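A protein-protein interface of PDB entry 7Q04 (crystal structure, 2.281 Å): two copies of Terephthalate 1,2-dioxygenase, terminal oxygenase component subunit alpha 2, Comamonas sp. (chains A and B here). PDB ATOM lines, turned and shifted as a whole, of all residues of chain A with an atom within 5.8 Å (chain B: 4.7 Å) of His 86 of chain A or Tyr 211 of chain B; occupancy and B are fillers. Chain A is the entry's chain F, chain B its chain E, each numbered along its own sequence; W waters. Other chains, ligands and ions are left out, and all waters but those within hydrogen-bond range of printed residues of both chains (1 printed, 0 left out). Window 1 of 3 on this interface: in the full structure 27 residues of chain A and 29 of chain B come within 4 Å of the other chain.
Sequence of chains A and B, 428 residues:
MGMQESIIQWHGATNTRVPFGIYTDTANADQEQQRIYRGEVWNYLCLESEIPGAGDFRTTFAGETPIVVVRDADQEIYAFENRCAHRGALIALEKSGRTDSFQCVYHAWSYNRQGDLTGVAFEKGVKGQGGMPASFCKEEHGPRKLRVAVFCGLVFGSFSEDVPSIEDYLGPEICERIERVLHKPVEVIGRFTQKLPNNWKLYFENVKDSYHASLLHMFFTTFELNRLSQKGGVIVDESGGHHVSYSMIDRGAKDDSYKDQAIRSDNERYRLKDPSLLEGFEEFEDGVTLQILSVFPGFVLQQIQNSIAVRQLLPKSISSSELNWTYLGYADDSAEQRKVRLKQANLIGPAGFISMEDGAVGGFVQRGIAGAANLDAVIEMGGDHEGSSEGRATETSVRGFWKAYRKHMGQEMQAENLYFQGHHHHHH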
ATOM      1  N   CYS A  84      24.443  -7.166 -25.165  1.00  0.00           N
ATOM      2  CA  CYS A  84      23.638  -6.156 -25.874  1.00  0.00           C
ATOM      3  C   CYS A  84      24.543  -4.953 -26.158  1.00  0.00           C
ATOM      4  O   CYS A  84      25.269  -4.518 -25.234  1.00  0.00           O
ATOM      5  CB  CYS A  84      22.430  -5.827 -25.019  1.00  0.00           C
ATOM      6  SG  CYS A  84      21.261  -4.641 -25.700  1.00  0.00           S
ATOM      7  N   ALA A  85      24.526  -4.457 -27.399  1.00  0.00           N
ATOM      8  CA  ALA A  85      25.399  -3.363 -27.866  1.00  0.00           C
ATOM      9  C   ALA A  85      24.877  -2.020 -27.337  1.00  0.00           C
ATOM     10  O   ALA A  85      25.465  -0.972 -27.626  1.00  0.00           O
ATOM     11  CB  ALA A  85      25.467  -3.384 -29.371  1.00  0.00           C
ATOM     12  N   HIS A  86      23.745  -2.021 -26.642  1.00  0.00           N
ATOM     13  CA  HIS A  86      23.217  -0.819 -25.949  1.00  0.00           C
ATOM     14  C   HIS A  86      24.067  -0.564 -24.700  1.00  0.00           C
ATOM     15  O   HIS A  86      25.113   0.127 -24.843  1.00  0.00           O
ATOM     16  CB  HIS A  86      21.712  -0.964 -25.683  1.00  0.00           C
ATOM     17  CG  HIS A  86      21.114   0.229 -25.039  1.00  0.00           C
ATOM     18  ND1 HIS A  86      20.117   0.131 -24.083  1.00  0.00           N
ATOM     19  CD2 HIS A  86      21.381   1.545 -25.189  1.00  0.00           C
ATOM     20  CE1 HIS A  86      19.778   1.346 -23.695  1.00  0.00           C
ATOM     21  NE2 HIS A  86      20.531   2.234 -24.353  1.00  0.00           N
ATOM     22  N   ARG A  87      23.653  -1.105 -23.548  1.00  0.00           N
ATOM     23  CA  ARG A  87      24.320  -0.862 -22.241  1.00  0.00           C
ATOM     24  C   ARG A  87      24.878  -2.171 -21.649  1.00  0.00           C
ATOM     25  O   ARG A  87      25.357  -2.113 -20.509  1.00  0.00           O
ATOM     26  CB  ARG A  87      23.376  -0.091 -21.310  1.00  0.00           C
ATOM     27  CG  ARG A  87      23.063   1.321 -21.819  1.00  0.00           C
ATOM     28  CD  ARG A  87      22.308   2.311 -20.910  1.00  0.00           C
ATOM     29  NE  ARG A  87      22.730   2.119 -19.549  1.00  0.00           N
ATOM     30  CZ  ARG A  87      21.942   1.740 -18.532  1.00  0.00           C
ATOM     31  NH1 ARG A  87      20.611   1.650 -18.661  1.00  0.00           N
ATOM     32  NH2 ARG A  87      22.546   1.450 -17.382  1.00  0.00           N
ATOM     33  N   GLY A  88      24.871  -3.286 -22.385  1.00  0.00           N
ATOM     34  CA  GLY A  88      25.755  -4.439 -22.114  1.00  0.00           C
ATOM     35  C   GLY A  88      25.053  -5.626 -21.471  1.00  0.00           C
ATOM     36  O   GLY A  88      25.748  -6.637 -21.197  1.00  0.00           O
ATOM     37  N   HIS A 107      15.778  -2.881 -22.779  1.00  0.00           N
ATOM     38  CA  HIS A 107      15.181  -1.856 -23.672  1.00  0.00           C
ATOM     39  C   HIS A 107      14.798  -2.432 -25.043  1.00  0.00           C
ATOM     40  O   HIS A 107      14.690  -1.651 -26.002  1.00  0.00           O
ATOM     41  CB  HIS A 107      16.149  -0.690 -23.860  1.00  0.00           C
ATOM     42  CG  HIS A 107      16.790  -0.228 -22.602  1.00  0.00           C
ATOM     43  ND1 HIS A 107      18.002  -0.726 -22.182  1.00  0.00           N
ATOM     44  CD2 HIS A 107      16.407   0.686 -21.694  1.00  0.00           C
ATOM     45  CE1 HIS A 107      18.338  -0.118 -21.063  1.00  0.00           C
ATOM     46  NE2 HIS A 107      17.382   0.769 -20.763  1.00  0.00           N
ATOM     47  N   TRP A 109      15.946  -4.167 -27.590  1.00  0.00           N
ATOM     48  CA  TRP A 109      16.749  -4.270 -28.832  1.00  0.00           C
ATOM     49  C   TRP A 109      16.713  -5.726 -29.351  1.00  0.00           C
ATOM     50  O   TRP A 109      16.982  -6.637 -28.567  1.00  0.00           O
ATOM     51  CB  TRP A 109      18.182  -3.772 -28.649  1.00  0.00           C
ATOM     52  CG  TRP A 109      18.306  -2.300 -28.456  1.00  0.00           C
ATOM     53  CD1 TRP A 109      17.368  -1.445 -27.965  1.00  0.00           C
ATOM     54  CD2 TRP A 109      19.484  -1.506 -28.662  1.00  0.00           C
ATOM     55  NE1 TRP A 109      17.879  -0.174 -27.835  1.00  0.00           N
ATOM     56  CE2 TRP A 109      19.171  -0.179 -28.272  1.00  0.00           C
ATOM     57  CE3 TRP A 109      20.768  -1.775 -29.163  1.00  0.00           C
ATOM     58  CZ2 TRP A 109      20.086   0.868 -28.372  1.00  0.00           C
ATOM     59  CZ3 TRP A 109      21.677  -0.736 -29.244  1.00  0.00           C
ATOM     60  CH2 TRP A 109      21.332   0.575 -28.882  1.00  0.00           C
ATOM     61  N   TYR A 111      17.948  -8.740 -32.072  1.00  0.00           N
ATOM     62  CA  TYR A 111      19.120  -9.297 -32.785  1.00  0.00           C
ATOM     63  C   TYR A 111      18.647 -10.518 -33.576  1.00  0.00           C
ATOM     64  O   TYR A 111      17.833 -11.257 -33.047  1.00  0.00           O
ATOM     65  CB  TYR A 111      20.239  -9.644 -31.799  1.00  0.00           C
ATOM     66  CG  TYR A 111      20.701  -8.459 -30.992  1.00  0.00           C
ATOM     67  CD1 TYR A 111      20.074  -8.103 -29.807  1.00  0.00           C
ATOM     68  CD2 TYR A 111      21.762  -7.677 -31.423  1.00  0.00           C
ATOM     69  CE1 TYR A 111      20.504  -7.001 -29.075  1.00  0.00           C
ATOM     70  CE2 TYR A 111      22.214  -6.586 -30.697  1.00  0.00           C
ATOM     71  CZ  TYR A 111      21.599  -6.252 -29.497  1.00  0.00           C
ATOM     72  OH  TYR A 111      22.049  -5.151 -28.801  1.00  0.00           O
ATOM     73  N   VAL A 120      15.472  -1.463 -32.597  1.00  0.00           N
ATOM     74  CA  VAL A 120      15.739  -0.594 -31.421  1.00  0.00           C
ATOM     75  C   VAL A 120      14.417  -0.001 -30.977  1.00  0.00           C
ATOM     76  O   VAL A 120      13.864   0.790 -31.698  1.00  0.00           O
ATOM     77  CB  VAL A 120      16.784   0.490 -31.740  1.00  0.00           C
ATOM     78  CG1 VAL A 120      16.897   1.517 -30.626  1.00  0.00           C
ATOM     79  CG2 VAL A 120      18.143  -0.125 -32.071  1.00  0.00           C
ATOM     80  N   ALA A 121      13.944  -0.380 -29.800  1.00  0.00           N
ATOM     81  CA  ALA A 121      12.659   0.133 -29.256  1.00  0.00           C
ATOM     82  C   ALA A 121      12.753   1.655 -29.222  1.00  0.00           C
ATOM     83  O   ALA A 121      13.804   2.173 -28.765  1.00  0.00           O
ATOM     84  CB  ALA A 121      12.360  -0.432 -27.893  1.00  0.00           C
ATOM     85  N   PHE A 122      11.726   2.310 -29.774  1.00  0.00           N
ATOM     86  CA  PHE A 122      11.558   3.782 -29.832  1.00  0.00           C
ATOM     87  C   PHE A 122      12.760   4.449 -30.531  1.00  0.00           C
ATOM     88  O   PHE A 122      13.151   5.572 -30.160  1.00  0.00           O
ATOM     89  CB  PHE A 122      11.411   4.337 -28.414  1.00  0.00           C
ATOM     90  CG  PHE A 122      10.352   3.702 -27.547  1.00  0.00           C
ATOM     91  CD1 PHE A 122       9.230   3.085 -28.094  1.00  0.00           C
ATOM     92  CD2 PHE A 122      10.450   3.802 -26.175  1.00  0.00           C
ATOM     93  CE1 PHE A 122       8.251   2.542 -27.278  1.00  0.00           C
ATOM     94  CE2 PHE A 122       9.474   3.247 -25.357  1.00  0.00           C
ATOM     95  CZ  PHE A 122       8.369   2.633 -25.912  1.00  0.00           C
ATOM     96  N   GLU A 123      13.351   3.801 -31.534  1.00  0.00           N
ATOM     97  CA  GLU A 123      14.483   4.395 -32.282  1.00  0.00           C
ATOM     98  C   GLU A 123      14.049   5.756 -32.855  1.00  0.00           C
ATOM     99  O   GLU A 123      14.915   6.689 -32.898  1.00  0.00           O
ATOM    100  CB  GLU A 123      14.925   3.477 -33.414  1.00  0.00           C
ATOM    101  CG  GLU A 123      16.181   3.961 -34.111  1.00  0.00           C
ATOM    102  CD  GLU A 123      16.682   3.026 -35.205  1.00  0.00           C
ATOM    103  OE1 GLU A 123      16.272   1.842 -35.255  1.00  0.00           O
ATOM    104  OE2 GLU A 123      17.494   3.481 -35.996  1.00  0.00           O
ATOM    105  N   MET A 132      16.516   8.174 -31.282  1.00  0.00           N
ATOM    106  CA  MET A 132      17.950   8.237 -31.636  1.00  0.00           C
ATOM    107  C   MET A 132      18.206   9.471 -32.483  1.00  0.00           C
ATOM    108  O   MET A 132      17.292   9.952 -33.152  1.00  0.00           O
ATOM    109  CB  MET A 132      18.363   6.961 -32.378  1.00  0.00           C
ATOM    110  CG  MET A 132      18.391   5.731 -31.421  1.00  0.00           C
ATOM    111  SD  MET A 132      19.536   6.012 -30.030  1.00  0.00           S
ATOM    112  CE  MET A 132      19.690   4.316 -29.470  1.00  0.00           C
ATOM    113  N   ASP B 209      16.589   5.748 -15.725  1.00  0.00           N
ATOM    114  CA  ASP B 209      16.416   5.204 -17.103  1.00  0.00           C
ATOM    115  C   ASP B 209      14.934   5.324 -17.464  1.00  0.00           C
ATOM    116  O   ASP B 209      14.204   4.363 -17.306  1.00  0.00           O
ATOM    117  CB  ASP B 209      16.978   3.779 -17.187  1.00  0.00           C
ATOM    118  CG  ASP B 209      17.084   3.150 -18.566  1.00  0.00           C
ATOM    119  OD1 ASP B 209      16.508   3.721 -19.535  1.00  0.00           O
ATOM    120  OD2 ASP B 209      17.752   2.073 -18.644  1.00  0.00           O
ATOM    121  N   SER B 210      14.530   6.492 -17.957  1.00  0.00           N
ATOM    122  CA  SER B 210      13.155   6.796 -18.432  1.00  0.00           C
ATOM    123  C   SER B 210      12.830   5.933 -19.667  1.00  0.00           C
ATOM    124  O   SER B 210      11.653   5.571 -19.855  1.00  0.00           O
ATOM    125  CB  SER B 210      13.013   8.274 -18.708  1.00  0.00           C
ATOM    126  OG  SER B 210      14.088   8.751 -19.519  1.00  0.00           O
ATOM    127  N   TYR B 211      13.831   5.589 -20.464  1.00  0.00           N
ATOM    128  CA  TYR B 211      13.694   4.713 -21.656  1.00  0.00           C
ATOM    129  C   TYR B 211      13.131   3.361 -21.199  1.00  0.00           C
ATOM    130  O   TYR B 211      12.103   2.904 -21.739  1.00  0.00           O
ATOM    131  CB  TYR B 211      15.047   4.682 -22.376  1.00  0.00           C
ATOM    132  CG  TYR B 211      15.172   3.850 -23.634  1.00  0.00           C
ATOM    133  CD1 TYR B 211      14.073   3.453 -24.404  1.00  0.00           C
ATOM    134  CD2 TYR B 211      16.450   3.543 -24.106  1.00  0.00           C
ATOM    135  CE1 TYR B 211      14.245   2.752 -25.585  1.00  0.00           C
ATOM    136  CE2 TYR B 211      16.640   2.802 -25.268  1.00  0.00           C
ATOM    137  CZ  TYR B 211      15.536   2.419 -26.025  1.00  0.00           C
ATOM    138  OH  TYR B 211      15.747   1.676 -27.162  1.00  0.00           O
ATOM    139  N   HIS B 212      13.790   2.736 -20.221  1.00  0.00           N
ATOM    140  CA  HIS B 212      13.344   1.457 -19.592  1.00  0.00           C
ATOM    141  C   HIS B 212      11.934   1.607 -19.002  1.00  0.00           C
ATOM    142  O   HIS B 212      11.064   0.754 -19.251  1.00  0.00           O
ATOM    143  CB  HIS B 212      14.343   0.994 -18.534  1.00  0.00           C
ATOM    144  CG  HIS B 212      13.826  -0.130 -17.706  1.00  0.00           C
ATOM    145  ND1 HIS B 212      13.467   0.024 -16.371  1.00  0.00           N
ATOM    146  CD2 HIS B 212      13.578  -1.428 -18.007  1.00  0.00           C
ATOM    147  CE1 HIS B 212      13.057  -1.136 -15.896  1.00  0.00           C
ATOM    148  NE2 HIS B 212      13.107  -2.039 -16.867  1.00  0.00           N
ATOM    149  N   ALA B 213      11.714   2.679 -18.243  1.00  0.00           N
ATOM    150  CA  ALA B 213      10.502   2.871 -17.413  1.00  0.00           C
ATOM    151  C   ALA B 213       9.306   3.082 -18.350  1.00  0.00           C
ATOM    152  O   ALA B 213       8.302   2.386 -18.186  1.00  0.00           O
ATOM    153  CB  ALA B 213      10.727   3.995 -16.430  1.00  0.00           C
ATOM    154  N   SER B 214       9.462   3.911 -19.375  1.00  0.00           N
ATOM    155  CA  SER B 214       8.414   4.142 -20.403  1.00  0.00           C
ATOM    156  C   SER B 214       8.162   2.830 -21.166  1.00  0.00           C
ATOM    157  O   SER B 214       6.998   2.503 -21.467  1.00  0.00           O
ATOM    158  CB  SER B 214       8.757   5.327 -21.308  1.00  0.00           C
ATOM    159  OG  SER B 214       9.818   5.076 -22.227  1.00  0.00           O
ATOM    160  N   LEU B 215       9.212   2.079 -21.468  1.00  0.00           N
ATOM    161  CA  LEU B 215       9.039   0.813 -22.225  1.00  0.00           C
ATOM    162  C   LEU B 215       8.086  -0.090 -21.429  1.00  0.00           C
ATOM    163  O   LEU B 215       7.153  -0.656 -21.981  1.00  0.00           O
ATOM    164  CB  LEU B 215      10.422   0.182 -22.416  1.00  0.00           C
ATOM    165  CG  LEU B 215      10.534  -0.873 -23.508  1.00  0.00           C
ATOM    166  CD1 LEU B 215       9.779  -0.504 -24.781  1.00  0.00           C
ATOM    167  CD2 LEU B 215      12.000  -1.098 -23.805  1.00  0.00           C
ATOM    168  N   ALA B 377      29.469   1.622 -23.180  1.00  0.00           N
ATOM    169  CA  ALA B 377      27.996   1.656 -23.277  1.00  0.00           C
ATOM    170  C   ALA B 377      27.602   2.761 -24.252  1.00  0.00           C
ATOM    171  O   ALA B 377      28.304   3.798 -24.277  1.00  0.00           O
ATOM    172  CB  ALA B 377      27.386   1.888 -21.916  1.00  0.00           C
ATOM    173  N   VAL B 378      26.510   2.564 -24.991  1.00  0.00           N
ATOM    174  CA  VAL B 378      25.985   3.584 -25.947  1.00  0.00           C
ATOM    175  C   VAL B 378      24.719   4.240 -25.379  1.00  0.00           C
ATOM    176  O   VAL B 378      23.717   3.533 -25.186  1.00  0.00           O
ATOM    177  CB  VAL B 378      25.728   2.926 -27.308  1.00  0.00           C
ATOM    178  CG1 VAL B 378      24.818   3.780 -28.172  1.00  0.00           C
ATOM    179  CG2 VAL B 378      27.042   2.587 -28.023  1.00  0.00           C
ATOM    180  N   MET B 381      20.053   8.199 -26.902  1.00  0.00           N
ATOM    181  CA  MET B 381      18.610   8.519 -26.865  1.00  0.00           C
ATOM    182  C   MET B 381      18.410   9.962 -26.368  1.00  0.00           C
ATOM    183  O   MET B 381      18.817  10.269 -25.222  1.00  0.00           O
ATOM    184  CB  MET B 381      17.949   7.527 -25.914  1.00  0.00           C
ATOM    185  CG  MET B 381      16.660   7.052 -26.423  1.00  0.00           C
ATOM    186  SD  MET B 381      16.876   6.062 -27.839  1.00  0.00           S
ATOM    187  CE  MET B 381      15.178   5.493 -27.959  1.00  0.00           C
ATOM    188  N   ARG B 392       9.665  10.595 -22.590  1.00  0.00           N
ATOM    189  CA  ARG B 392      10.558   9.747 -21.763  1.00  0.00           C
ATOM    190  C   ARG B 392      11.431   8.822 -22.614  1.00  0.00           C
ATOM    191  O   ARG B 392      12.292   8.155 -21.988  1.00  0.00           O
ATOM    192  CB  ARG B 392       9.688   8.987 -20.764  1.00  0.00           C
ATOM    193  CG  ARG B 392       9.234   9.889 -19.624  1.00  0.00           C
ATOM    194  CD  ARG B 392       8.520   9.120 -18.535  1.00  0.00           C
ATOM    195  NE  ARG B 392       7.315   8.413 -18.963  1.00  0.00           N
ATOM    196  CZ  ARG B 392       6.739   7.445 -18.254  1.00  0.00           C
ATOM    197  NH1 ARG B 392       7.313   7.023 -17.128  1.00  0.00           N
ATOM    198  NH2 ARG B 392       5.630   6.866 -18.698  1.00  0.00           N
ATOM    199  N   THR B 394      14.181   8.976 -23.957  1.00  0.00           N
ATOM    200  CA  THR B 394      15.469   9.713 -23.862  1.00  0.00           C
ATOM    201  C   THR B 394      16.330   9.072 -22.762  1.00  0.00           C
ATOM    202  O   THR B 394      15.763   8.334 -21.925  1.00  0.00           O
ATOM    203  CB  THR B 394      15.228  11.187 -23.558  1.00  0.00           C
ATOM    204  OG1 THR B 394      16.478  11.861 -23.394  1.00  0.00           O
ATOM    205  CG2 THR B 394      14.408  11.359 -22.319  1.00  0.00           C
ATOM    206  N   GLU B 395      17.629   9.378 -22.745  1.00  0.00           N
ATOM    207  CA  GLU B 395      18.588   8.944 -21.703  1.00  0.00           C
ATOM    208  C   GLU B 395      19.282  10.171 -21.104  1.00  0.00           C
ATOM    209  O   GLU B 395      20.383  10.039 -20.586  1.00  0.00           O
ATOM    210  CB  GLU B 395      19.575   7.955 -22.322  1.00  0.00           C
ATOM    211  CG  GLU B 395      18.964   6.585 -22.589  1.00  0.00           C
ATOM    212  CD  GLU B 395      19.811   5.696 -23.504  1.00  0.00           C
ATOM    213  OE1 GLU B 395      20.455   6.236 -24.456  1.00  0.00           O
ATOM    214  OE2 GLU B 395      19.818   4.459 -23.323  1.00  0.00           O
HETATM  215  O   HOH W   1      21.547   4.844 -26.288  1.00  0.00           O
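NH1 of Arg 87 of chain A is in salt-bridge range of OD2 of Asp 209 of chain B, at 2.9 Å. OD2 of Asp 209 of chain B lies within hydrogen-bond range of NE2 of His 107 of chain A (2.5 Å). The indole nitrogen (NE1) of Trp 109 of chain A sits at hydrogen-bond distance from the side-chain hydroxyl (OH) of Tyr 211 of chain B (2.9 Å). OH of Tyr 211 of chain B lies within hydrogen-bond range of O of Ala 121 of chain A, at 2.6 Å. The backbone carbonyl oxygen (O) of His 86 of chain A lies within hydrogen-bond range of the backbone NH (N) of Val 378 of chain B. NE2 of His 86 of chain A lies within hydrogen-bond range of OE2 of Glu 395 of chain B. SD of Met 381 of chain B lies close to SD of Met 132 of chain A.
The backbone NH (N) of His 212 of chain B sits at hydrogen-bond distance from the side-chain carboxylate (OD1) of Asp 209 of chain B, at 3.0 Å. The side-chain hydroxyl of Ser 214 of chain B lies within hydrogen-bond range of the backbone carbonyl oxygen of Ser 210 of chain B. The backbone carbonyl oxygen of Met 381 of chain B is in hydrogen-bond range of the backbone NH of Glu 395 of chain B (2.9 Å). The backbone NH of His 86 of chain A sits close to the side-chain sulfur of Cys 84 of chain A. The backbone NH (N) of Ala 85 of chain A lies within hydrogen-bond range of the side-chain hydroxyl (OH) of Tyr 111 of chain A. The backbone NH (N) of Met 132 of chain A is in hydrogen-bond range of the backbone carbonyl oxygen (O) of Glu 123 of chain A, at 2.7 Å.
Val 378 of chain B touches Ala 85 of chain A (CG2 to O, 3.9 Å). Tyr 211 of chain B touches His 86 of chain A (CE2 to CE1, 3.8 Å). His 107 of chain A touches His 212 of chain B (CD2 to N, 3.6 Å). Leu 215 of chain B touches His 107 of chain A. Tyr 211 of chain B touches Val 120 of chain A. Met 381 of chain B touches Ala 121 of chain A. CE1 of Tyr 211 of chain B touches CD2 of Phe 122 of chain A (3.98 Å). Ser 214 of chain B touches Phe 122 of chain A. CZ of Phe 122 of chain A touches CD1 of Leu 215 of chain B (3.6 Å). CE of Met 381 of chain B touches O of Phe 122 of chain A, at 3.0 Å.
Printed residues of chain B within 4 Å of His 86 of chain A: Tyr 211, Ala 377, Val 378 and Glu 395. Printed residues of chain A within 4 Å of Tyr 211 of chain B: His 86, His 107, Trp 109, Val 120, Ala 121 and Phe 122. Printed residues of chain B within 4 Å of Phe 122 of chain A: Tyr 211, Ser 214, Leu 215 and Met 381. Of the printed residues of chain A, Glu 395 of chain B touches His 86 (2.6 Å). Gly 88 of chain A touches none of the printed residues of chain B. Arg 392 of chain B touches none of the printed residues of chain A. The nearest printed residue of chain B that does not touch His 86 of chain A is Asp 209 of chain B (5.5 Å). The nearest printed residue of chain A that does not touch Tyr 211 of chain B is Met 132 of chain A (5.3 Å).
Of the 13 printed residues of chain B, 9 touch a printed residue of chain A. Printed residues of chain B that touch a printed residue of chain A: Asp 209, Tyr 211, His 212, Ser 214, Leu 215, Ala 377, Val 378, Met 381 and Glu 395. Of the 13 printed residues of chain A, 9 touch a printed residue of chain B. Among the printed residues, 19 pairs touch across the chains. Among the printed residues, Asp or Glu carboxylates within 4 Å of a Lys or Arg side-chain nitrogen of the other chain: Arg 87 of chain A with Asp 209 of chain B.
No position is printed for both chains.
Water W1 lies within hydrogen-bond range of the side-chain carboxylate (OE1) of Glu 395 of chain B (2.5 Å), the backbone carbonyl oxygen (O) of Val 378 of chain B (2.8 Å) and a ring nitrogen (NE2) of His 86 of chain A (3.4 Å).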
